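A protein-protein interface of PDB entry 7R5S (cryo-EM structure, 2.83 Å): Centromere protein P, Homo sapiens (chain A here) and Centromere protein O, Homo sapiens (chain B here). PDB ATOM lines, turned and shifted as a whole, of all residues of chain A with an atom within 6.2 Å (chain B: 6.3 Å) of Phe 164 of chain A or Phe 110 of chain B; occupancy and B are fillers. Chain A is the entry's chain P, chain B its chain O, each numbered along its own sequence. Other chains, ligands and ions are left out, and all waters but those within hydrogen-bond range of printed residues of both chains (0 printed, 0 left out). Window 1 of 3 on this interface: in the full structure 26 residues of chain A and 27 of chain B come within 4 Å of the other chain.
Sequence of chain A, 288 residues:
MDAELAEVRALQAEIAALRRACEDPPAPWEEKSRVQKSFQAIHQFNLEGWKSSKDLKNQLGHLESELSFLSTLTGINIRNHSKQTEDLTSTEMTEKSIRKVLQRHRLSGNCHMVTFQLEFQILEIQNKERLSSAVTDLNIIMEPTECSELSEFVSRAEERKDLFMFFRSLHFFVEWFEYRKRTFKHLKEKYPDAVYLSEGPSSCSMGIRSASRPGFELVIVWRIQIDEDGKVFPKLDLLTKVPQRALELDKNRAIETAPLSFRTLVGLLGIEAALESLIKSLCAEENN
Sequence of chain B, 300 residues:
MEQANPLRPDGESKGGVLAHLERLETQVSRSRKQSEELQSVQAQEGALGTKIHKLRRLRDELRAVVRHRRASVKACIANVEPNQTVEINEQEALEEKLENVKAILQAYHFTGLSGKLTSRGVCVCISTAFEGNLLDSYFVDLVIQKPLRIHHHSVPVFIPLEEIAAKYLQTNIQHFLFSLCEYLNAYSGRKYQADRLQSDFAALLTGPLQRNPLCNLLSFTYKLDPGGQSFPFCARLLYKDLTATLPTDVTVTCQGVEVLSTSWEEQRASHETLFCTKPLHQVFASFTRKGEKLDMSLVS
NE2 of His 81 of chain A is in hydrogen-bond range of ND1 of His 105 of chain A. N of Ser 127 of chain B lies within hydrogen-bond range of O of Gly 112 of chain B (3.0 Å). N of Ala 129 of chain B is in hydrogen-bond range of OD1 of Asn 185 of chain B.
Of the 15 printed residues of chain B, 8 touch a printed residue of chain A. Hydrophobic or aromatic side chains of chain B within 4 Å of the printed part of chain A: Ala 107 and Ala 129. Hydrophobic or aromatic side chains of chain A within 4 Å of the printed part of chain B: His 81, Leu 163, Phe 164 and Phe 167. Among the printed residues, 10 pairs touch across the chains.
CG of His 81 of chain A touches CB of Ala 107 of chain B (3.5 Å). Leu 163 of chain A touches Phe 110 of chain B. Phe 164 of chain A touches Phe 110 of chain B. Thr 111 of chain B touches Phe 164 of chain A (O to CD1, 3.8 Å). Phe 164 of chain A touches Gly 112 of chain B. CD2 of Phe 164 of chain A touches O of Ser 127 of chain B, 3.8 Å away. CE2 of Phe 164 of chain A touches C of Thr 128 of chain B, 3.8 Å away. Phe 164 of chain A touches Ala 129 of chain B (CE2 to CB, 3.6 Å). Phe 167 of chain A touches Thr 111 of chain B (CD2 to O, 3.5 Å).
ND2 of Asn 185 of chain B sits close to NH1 of Arg 168 of chain A (3.0 Å).
Of chain B, only Phe 110, Thr 111, Gly 112, Ser 127, Thr 128 and Ala 129 come within 4 Å of Phe 164 of chain A. Of chain A, only Leu 163 (3.9 Å) and Phe 164 (3.4 Å) come within 4 Å of Phe 110 of chain B. Of the printed residues of chain A, Asn 185 of chain B touches Arg 168. Of the printed residues of chain B, His 81 of chain A touches Ala 107 (3.5 Å). Of the printed residues of chain A, Thr 128 of chain B touches Phe 164. Of the printed residues of chain B, Phe 167 of chain A touches Thr 111. Printed residues of chain A within 4 Å of Ala 129 of chain B: Phe 164. Phe 166 of chain A touches none of the printed residues of chain B. The nearest residue of chain A that does not touch Phe 110 of chain B is Phe 120 of chain A (4.03 Å). The nearest printed residue of chain A that does not touch Gly 112 of chain B is Phe 167 of chain A (5.5 Å).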
ATOM      1  N   HIS A  81      22.757  22.336  13.789  1.00  0.00           N
ATOM      2  CA  HIS A  81      22.567  22.024  12.381  1.00  0.00           C
ATOM      3  C   HIS A  81      21.326  22.736  11.868  1.00  0.00           C
ATOM      4  O   HIS A  81      20.290  22.755  12.537  1.00  0.00           O
ATOM      5  CB  HIS A  81      22.437  20.510  12.163  1.00  0.00           C
ATOM      6  CG  HIS A  81      21.948  20.133  10.799  1.00  0.00           C
ATOM      7  ND1 HIS A  81      20.756  19.473  10.594  1.00  0.00           N
ATOM      8  CD2 HIS A  81      22.493  20.319   9.573  1.00  0.00           C
ATOM      9  CE1 HIS A  81      20.586  19.270   9.300  1.00  0.00           C
ATOM     10  NE2 HIS A  81      21.624  19.774   8.658  1.00  0.00           N
ATOM     11  N   GLN A 103      17.903  20.950  -0.909  1.00  0.00           N
ATOM     12  CA  GLN A 103      18.068  21.001   0.538  1.00  0.00           C
ATOM     13  C   GLN A 103      19.433  21.589   0.862  1.00  0.00           C
ATOM     14  O   GLN A 103      20.462  20.999   0.519  1.00  0.00           O
ATOM     15  CB  GLN A 103      17.923  19.609   1.155  1.00  0.00           C
ATOM     16  CG  GLN A 103      16.604  18.927   0.837  1.00  0.00           C
ATOM     17  CD  GLN A 103      16.536  17.514   1.378  1.00  0.00           C
ATOM     18  OE1 GLN A 103      17.507  17.003   1.937  1.00  0.00           O
ATOM     19  NE2 GLN A 103      15.386  16.871   1.214  1.00  0.00           N
ATOM     20  N   HIS A 105      21.995  22.419   3.704  1.00  0.00           N
ATOM     21  CA  HIS A 105      22.364  22.064   5.064  1.00  0.00           C
ATOM     22  C   HIS A 105      23.585  22.862   5.501  1.00  0.00           C
ATOM     23  O   HIS A 105      24.438  23.227   4.685  1.00  0.00           O
ATOM     24  CB  HIS A 105      22.658  20.566   5.186  1.00  0.00           C
ATOM     25  CG  HIS A 105      21.570  19.690   4.649  1.00  0.00           C
ATOM     26  ND1 HIS A 105      20.662  19.046   5.463  1.00  0.00           N
ATOM     27  CD2 HIS A 105      21.244  19.348   3.380  1.00  0.00           C
ATOM     28  CE1 HIS A 105      19.825  18.345   4.718  1.00  0.00           C
ATOM     29  NE2 HIS A 105      20.156  18.513   3.450  1.00  0.00           N
ATOM     30  N   LEU A 107      26.304  23.015   9.088  1.00  0.00           N
ATOM     31  CA  LEU A 107      26.621  22.473  10.402  1.00  0.00           C
ATOM     32  C   LEU A 107      28.077  22.753  10.739  1.00  0.00           C
ATOM     33  O   LEU A 107      28.939  22.787   9.859  1.00  0.00           O
ATOM     34  CB  LEU A 107      26.325  20.968  10.470  1.00  0.00           C
ATOM     35  CG  LEU A 107      27.205  19.978   9.700  1.00  0.00           C
ATOM     36  CD1 LEU A 107      28.342  19.442  10.562  1.00  0.00           C
ATOM     37  CD2 LEU A 107      26.365  18.836   9.148  1.00  0.00           C
ATOM     38  N   PHE A 120      26.535  23.006   2.666  1.00  0.00           N
ATOM     39  CA  PHE A 120      26.403  22.370   1.365  1.00  0.00           C
ATOM     40  C   PHE A 120      24.937  22.347   0.962  1.00  0.00           C
ATOM     41  O   PHE A 120      24.053  22.752   1.720  1.00  0.00           O
ATOM     42  CB  PHE A 120      26.992  20.952   1.367  1.00  0.00           C
ATOM     43  CG  PHE A 120      26.315  20.007   2.319  1.00  0.00           C
ATOM     44  CD1 PHE A 120      26.646  19.999   3.663  1.00  0.00           C
ATOM     45  CD2 PHE A 120      25.358  19.114   1.865  1.00  0.00           C
ATOM     46  CE1 PHE A 120      26.028  19.128   4.539  1.00  0.00           C
ATOM     47  CE2 PHE A 120      24.738  18.240   2.737  1.00  0.00           C
ATOM     48  CZ  PHE A 120      25.075  18.246   4.074  1.00  0.00           C
ATOM     49  N   ILE A 122      22.146  19.784  -1.487  1.00  0.00           N
ATOM     50  CA  ILE A 122      21.904  18.570  -2.251  1.00  0.00           C
ATOM     51  C   ILE A 122      20.623  18.738  -3.056  1.00  0.00           C
ATOM     52  O   ILE A 122      19.721  19.498  -2.684  1.00  0.00           O
ATOM     53  CB  ILE A 122      21.820  17.322  -1.345  1.00  0.00           C
ATOM     54  CG1 ILE A 122      20.667  17.459  -0.349  1.00  0.00           C
ATOM     55  CG2 ILE A 122      23.133  17.106  -0.613  1.00  0.00           C
ATOM     56  CD1 ILE A 122      20.499  16.258   0.555  1.00  0.00           C
ATOM     57  N   ASP A 162      33.136  16.029  -2.089  1.00  0.00           N
ATOM     58  CA  ASP A 162      33.013  14.778  -1.355  1.00  0.00           C
ATOM     59  C   ASP A 162      32.989  15.075   0.136  1.00  0.00           C
ATOM     60  O   ASP A 162      33.682  15.982   0.607  1.00  0.00           O
ATOM     61  CB  ASP A 162      34.161  13.816  -1.686  1.00  0.00           C
ATOM     62  CG  ASP A 162      33.832  12.377  -1.342  1.00  0.00           C
ATOM     63  OD1 ASP A 162      32.709  12.122  -0.857  1.00  0.00           O
ATOM     64  OD2 ASP A 162      34.693  11.500  -1.561  1.00  0.00           O
ATOM     65  N   LEU A 163      32.192  14.309   0.875  1.00  0.00           N
ATOM     66  CA  LEU A 163      31.954  14.563   2.291  1.00  0.00           C
ATOM     67  C   LEU A 163      32.579  13.532   3.216  1.00  0.00           C
ATOM     68  O   LEU A 163      33.144  13.903   4.247  1.00  0.00           O
ATOM     69  CB  LEU A 163      30.446  14.630   2.563  1.00  0.00           C
ATOM     70  CG  LEU A 163      29.984  15.594   3.657  1.00  0.00           C
ATOM     71  CD1 LEU A 163      30.345  17.026   3.294  1.00  0.00           C
ATOM     72  CD2 LEU A 163      28.488  15.458   3.890  1.00  0.00           C
ATOM     73  N   PHE A 164      32.501  12.245   2.876  1.00  0.00           N
ATOM     74  CA  PHE A 164      32.980  11.205   3.782  1.00  0.00           C
ATOM     75  C   PHE A 164      34.502  11.111   3.778  1.00  0.00           C
ATOM     76  O   PHE A 164      35.122  10.956   4.841  1.00  0.00           O
ATOM     77  CB  PHE A 164      32.364   9.857   3.405  1.00  0.00           C
ATOM     78  CG  PHE A 164      30.861   9.872   3.329  1.00  0.00           C
ATOM     79  CD1 PHE A 164      30.118  10.724   4.130  1.00  0.00           C
ATOM     80  CD2 PHE A 164      30.192   9.030   2.457  1.00  0.00           C
ATOM     81  CE1 PHE A 164      28.738  10.737   4.060  1.00  0.00           C
ATOM     82  CE2 PHE A 164      28.812   9.039   2.384  1.00  0.00           C
ATOM     83  CZ  PHE A 164      28.085   9.892   3.186  1.00  0.00           C
ATOM     84  N   MET A 165      35.114  11.190   2.594  1.00  0.00           N
ATOM     85  CA  MET A 165      36.569  11.137   2.501  1.00  0.00           C
ATOM     86  C   MET A 165      37.211  12.266   3.296  1.00  0.00           C
ATOM     87  O   MET A 165      38.279  12.086   3.893  1.00  0.00           O
ATOM     88  CB  MET A 165      36.999  11.196   1.036  1.00  0.00           C
ATOM     89  CG  MET A 165      38.500  11.117   0.818  1.00  0.00           C
ATOM     90  SD  MET A 165      38.948  11.228  -0.923  1.00  0.00           S
ATOM     91  CE  MET A 165      38.264  12.827  -1.347  1.00  0.00           C
ATOM     92  N   PHE A 166      36.567  13.435   3.320  1.00  0.00           N
ATOM     93  CA  PHE A 166      37.071  14.548   4.117  1.00  0.00           C
ATOM     94  C   PHE A 166      37.149  14.173   5.591  1.00  0.00           C
ATOM     95  O   PHE A 166      38.173  14.394   6.246  1.00  0.00           O
ATOM     96  CB  PHE A 166      36.182  15.777   3.915  1.00  0.00           C
ATOM     97  CG  PHE A 166      36.356  16.832   4.969  1.00  0.00           C
ATOM     98  CD1 PHE A 166      37.473  17.651   4.971  1.00  0.00           C
ATOM     99  CD2 PHE A 166      35.401  17.010   5.956  1.00  0.00           C
ATOM    100  CE1 PHE A 166      37.635  18.623   5.939  1.00  0.00           C
ATOM    101  CE2 PHE A 166      35.557  17.980   6.927  1.00  0.00           C
ATOM    102  CZ  PHE A 166      36.676  18.789   6.918  1.00  0.00           C
ATOM    103  N   PHE A 167      36.073  13.590   6.127  1.00  0.00           N
ATOM    104  CA  PHE A 167      36.064  13.208   7.537  1.00  0.00           C
ATOM    105  C   PHE A 167      37.087  12.116   7.825  1.00  0.00           C
ATOM    106  O   PHE A 167      37.773  12.158   8.853  1.00  0.00           O
ATOM    107  CB  PHE A 167      34.664  12.753   7.951  1.00  0.00           C
ATOM    108  CG  PHE A 167      33.707  13.884   8.198  1.00  0.00           C
ATOM    109  CD1 PHE A 167      33.861  14.710   9.299  1.00  0.00           C
ATOM    110  CD2 PHE A 167      32.650  14.116   7.336  1.00  0.00           C
ATOM    111  CE1 PHE A 167      32.982  15.751   9.531  1.00  0.00           C
ATOM    112  CE2 PHE A 167      31.766  15.154   7.563  1.00  0.00           C
ATOM    113  CZ  PHE A 167      31.933  15.972   8.662  1.00  0.00           C
ATOM    114  N   ARG A 168      37.206  11.131   6.930  1.00  0.00           N
ATOM    115  CA  ARG A 168      38.173  10.056   7.147  1.00  0.00           C
ATOM    116  C   ARG A 168      39.599  10.595   7.168  1.00  0.00           C
ATOM    117  O   ARG A 168      40.395  10.262   8.060  1.00  0.00           O
ATOM    118  CB  ARG A 168      38.019   8.985   6.067  1.00  0.00           C
ATOM    119  CG  ARG A 168      36.642   8.347   6.013  1.00  0.00           C
ATOM    120  CD  ARG A 168      36.675   7.029   5.256  1.00  0.00           C
ATOM    121  NE  ARG A 168      37.382   7.144   3.984  1.00  0.00           N
ATOM    122  CZ  ARG A 168      36.803   7.473   2.834  1.00  0.00           C
ATOM    123  NH1 ARG A 168      35.503   7.726   2.791  1.00  0.00           N
ATOM    124  NH2 ARG A 168      37.525   7.552   1.724  1.00  0.00           N
ATOM    125  N   SER A 169      39.941  11.435   6.188  1.00  0.00           N
ATOM    126  CA  SER A 169      41.283  11.999   6.135  1.00  0.00           C
ATOM    127  C   SER A 169      41.544  12.910   7.325  1.00  0.00           C
ATOM    128  O   SER A 169      42.660  12.942   7.849  1.00  0.00           O
ATOM    129  CB  SER A 169      41.481  12.764   4.832  1.00  0.00           C
ATOM    130  OG  SER A 169      40.999  14.085   4.971  1.00  0.00           O
ATOM    131  N   LEU B 105      21.171  14.280  16.161  1.00  0.00           N
ATOM    132  CA  LEU B 105      21.440  12.901  15.757  1.00  0.00           C
ATOM    133  C   LEU B 105      21.232  12.711  14.256  1.00  0.00           C
ATOM    134  O   LEU B 105      22.023  12.025  13.592  1.00  0.00           O
ATOM    135  CB  LEU B 105      20.555  11.939  16.549  1.00  0.00           C
ATOM    136  CG  LEU B 105      21.187  11.264  17.769  1.00  0.00           C
ATOM    137  CD1 LEU B 105      21.800  12.290  18.710  1.00  0.00           C
ATOM    138  CD2 LEU B 105      20.161  10.414  18.501  1.00  0.00           C
ATOM    139  N   GLN B 106      20.175  13.313  13.703  1.00  0.00           N
ATOM    140  CA  GLN B 106      19.936  13.204  12.268  1.00  0.00           C
ATOM    141  C   GLN B 106      21.063  13.837  11.461  1.00  0.00           C
ATOM    142  O   GLN B 106      21.386  13.360  10.368  1.00  0.00           O
ATOM    143  CB  GLN B 106      18.596  13.847  11.907  1.00  0.00           C
ATOM    144  CG  GLN B 106      17.420  12.880  11.906  1.00  0.00           C
ATOM    145  CD  GLN B 106      17.181  12.247  13.263  1.00  0.00           C
ATOM    146  OE1 GLN B 106      17.718  11.182  13.568  1.00  0.00           O
ATOM    147  NE2 GLN B 106      16.370  12.901  14.085  1.00  0.00           N
ATOM    148  N   ALA B 107      21.671  14.905  11.981  1.00  0.00           N
ATOM    149  CA  ALA B 107      22.806  15.516  11.298  1.00  0.00           C
ATOM    150  C   ALA B 107      24.080  14.702  11.494  1.00  0.00           C
ATOM    151  O   ALA B 107      24.924  14.641  10.594  1.00  0.00           O
ATOM    152  CB  ALA B 107      23.006  16.949  11.790  1.00  0.00           C
ATOM    153  N   TYR B 108      24.236  14.081  12.666  1.00  0.00           N
ATOM    154  CA  TYR B 108      25.364  13.185  12.892  1.00  0.00           C
ATOM    155  C   TYR B 108      25.316  11.993  11.949  1.00  0.00           C
ATOM    156  O   TYR B 108      26.360  11.431  11.603  1.00  0.00           O
ATOM    157  CB  TYR B 108      25.367  12.707  14.344  1.00  0.00           C
ATOM    158  CG  TYR B 108      26.738  12.393  14.887  1.00  0.00           C
ATOM    159  CD1 TYR B 108      27.432  13.325  15.644  1.00  0.00           C
ATOM    160  CD2 TYR B 108      27.340  11.167  14.644  1.00  0.00           C
ATOM    161  CE1 TYR B 108      28.684  13.047  16.145  1.00  0.00           C
ATOM    162  CE2 TYR B 108      28.596  10.879  15.139  1.00  0.00           C
ATOM    163  CZ  TYR B 108      29.263  11.824  15.890  1.00  0.00           C
ATOM    164  OH  TYR B 108      30.514  11.549  16.390  1.00  0.00           O
ATOM    165  N   HIS B 109      24.113  11.590  11.538  1.00  0.00           N
ATOM    166  CA  HIS B 109      23.988  10.527  10.546  1.00  0.00           C
ATOM    167  C   HIS B 109      24.692  10.884   9.239  1.00  0.00           C
ATOM    168  O   HIS B 109      25.106   9.989   8.492  1.00  0.00           O
ATOM    169  CB  HIS B 109      22.510  10.225  10.290  1.00  0.00           C
ATOM    170  CG  HIS B 109      22.262   9.396   9.068  1.00  0.00           C
ATOM    171  ND1 HIS B 109      22.015   9.949   7.830  1.00  0.00           N
ATOM    172  CD2 HIS B 109      22.226   8.053   8.894  1.00  0.00           C
ATOM    173  CE1 HIS B 109      21.835   8.983   6.947  1.00  0.00           C
ATOM    174  NE2 HIS B 109      21.958   7.823   7.567  1.00  0.00           N
ATOM    175  N   PHE B 110      24.851  12.178   8.952  1.00  0.00           N
ATOM    176  CA  PHE B 110      25.431  12.632   7.692  1.00  0.00           C
ATOM    177  C   PHE B 110      26.952  12.542   7.650  1.00  0.00           C
ATOM    178  O   PHE B 110      27.531  12.724   6.574  1.00  0.00           O
ATOM    179  CB  PHE B 110      25.012  14.079   7.415  1.00  0.00           C
ATOM    180  CG  PHE B 110      23.833  14.207   6.495  1.00  0.00           C
ATOM    181  CD1 PHE B 110      22.544  14.027   6.967  1.00  0.00           C
ATOM    182  CD2 PHE B 110      24.014  14.516   5.157  1.00  0.00           C
ATOM    183  CE1 PHE B 110      21.458  14.147   6.122  1.00  0.00           C
ATOM    184  CE2 PHE B 110      22.933  14.637   4.306  1.00  0.00           C
ATOM    185  CZ  PHE B 110      21.652  14.453   4.790  1.00  0.00           C
ATOM    186  N   THR B 111      27.613  12.273   8.778  1.00  0.00           N
ATOM    187  CA  THR B 111      29.072  12.304   8.810  1.00  0.00           C
ATOM    188  C   THR B 111      29.711  11.121   8.094  1.00  0.00           C
ATOM    189  O   THR B 111      30.919  11.161   7.833  1.00  0.00           O
ATOM    190  CB  THR B 111      29.571  12.355  10.255  1.00  0.00           C
ATOM    191  OG1 THR B 111      30.947  12.757  10.269  1.00  0.00           O
ATOM    192  CG2 THR B 111      29.451  10.989  10.910  1.00  0.00           C
ATOM    193  N   GLY B 112      28.947  10.080   7.775  1.00  0.00           N
ATOM    194  CA  GLY B 112      29.498   8.922   7.099  1.00  0.00           C
ATOM    195  C   GLY B 112      29.235   7.628   7.839  1.00  0.00           C
ATOM    196  O   GLY B 112      28.997   6.587   7.218  1.00  0.00           O
ATOM    197  N   LEU B 113      29.273   7.682   9.168  1.00  0.00           N
ATOM    198  CA  LEU B 113      28.988   6.525  10.001  1.00  0.00           C
ATOM    199  C   LEU B 113      28.174   6.969  11.207  1.00  0.00           C
ATOM    200  O   LEU B 113      28.482   7.986  11.835  1.00  0.00           O
ATOM    201  CB  LEU B 113      30.275   5.815  10.455  1.00  0.00           C
ATOM    202  CG  LEU B 113      31.258   6.529  11.387  1.00  0.00           C
ATOM    203  CD1 LEU B 113      32.089   5.512  12.151  1.00  0.00           C
ATOM    204  CD2 LEU B 113      32.164   7.475  10.614  1.00  0.00           C
ATOM    205  N   SER B 114      27.129   6.208  11.514  1.00  0.00           N
ATOM    206  CA  SER B 114      26.242   6.509  12.628  1.00  0.00           C
ATOM    207  C   SER B 114      26.098   5.274  13.506  1.00  0.00           C
ATOM    208  O   SER B 114      26.475   4.166  13.121  1.00  0.00           O
ATOM    209  CB  SER B 114      24.867   6.982  12.138  1.00  0.00           C
ATOM    210  OG  SER B 114      24.002   5.883  11.909  1.00  0.00           O
ATOM    211  N   SER B 127      27.706   4.568   5.469  1.00  0.00           N
ATOM    212  CA  SER B 127      27.211   5.118   4.217  1.00  0.00           C
ATOM    213  C   SER B 127      28.352   5.254   3.217  1.00  0.00           C
ATOM    214  O   SER B 127      29.510   5.455   3.594  1.00  0.00           O
ATOM    215  CB  SER B 127      26.547   6.481   4.437  1.00  0.00           C
ATOM    216  OG  SER B 127      25.489   6.387   5.375  1.00  0.00           O
ATOM    217  N   THR B 128      28.013   5.145   1.934  1.00  0.00           N
ATOM    218  CA  THR B 128      28.989   5.214   0.857  1.00  0.00           C
ATOM    219  C   THR B 128      28.563   6.261  -0.162  1.00  0.00           C
ATOM    220  O   THR B 128      27.371   6.490  -0.381  1.00  0.00           O
ATOM    221  CB  THR B 128      29.162   3.857   0.159  1.00  0.00           C
ATOM    222  OG1 THR B 128      27.896   3.411  -0.343  1.00  0.00           O
ATOM    223  CG2 THR B 128      29.710   2.823   1.128  1.00  0.00           C
ATOM    224  N   ALA B 129      29.555   6.890  -0.788  1.00  0.00           N
ATOM    225  CA  ALA B 129      29.309   7.908  -1.800  1.00  0.00           C
ATOM    226  C   ALA B 129      30.567   8.089  -2.634  1.00  0.00           C
ATOM    227  O   ALA B 129      31.685   7.944  -2.132  1.00  0.00           O
ATOM    228  CB  ALA B 129      28.891   9.242  -1.172  1.00  0.00           C
ATOM    229  N   LEU B 134      25.408   9.916  -3.676  1.00  0.00           N
ATOM    230  CA  LEU B 134      25.130   9.005  -2.575  1.00  0.00           C
ATOM    231  C   LEU B 134      24.766   7.621  -3.099  1.00  0.00           C
ATOM    232  O   LEU B 134      24.192   7.470  -4.181  1.00  0.00           O
ATOM    233  CB  LEU B 134      23.999   9.548  -1.700  1.00  0.00           C
ATOM    234  CG  LEU B 134      24.392  10.490  -0.557  1.00  0.00           C
ATOM    235  CD1 LEU B 134      24.925  11.817  -1.083  1.00  0.00           C
ATOM    236  CD2 LEU B 134      23.215  10.714   0.379  1.00  0.00           C
ATOM    237  N   ASN B 185      33.680   2.064   0.743  1.00  0.00           N
ATOM    238  CA  ASN B 185      33.686   3.213  -0.156  1.00  0.00           C
ATOM    239  C   ASN B 185      34.423   2.898  -1.450  1.00  0.00           C
ATOM    240  O   ASN B 185      33.958   3.256  -2.538  1.00  0.00           O
ATOM    241  CB  ASN B 185      34.312   4.420   0.540  1.00  0.00           C
ATOM    242  CG  ASN B 185      33.319   5.176   1.397  1.00  0.00           C
ATOM    243  OD1 ASN B 185      32.256   5.577   0.926  1.00  0.00           O
ATOM    244  ND2 ASN B 185      33.659   5.371   2.665  1.00  0.00           N
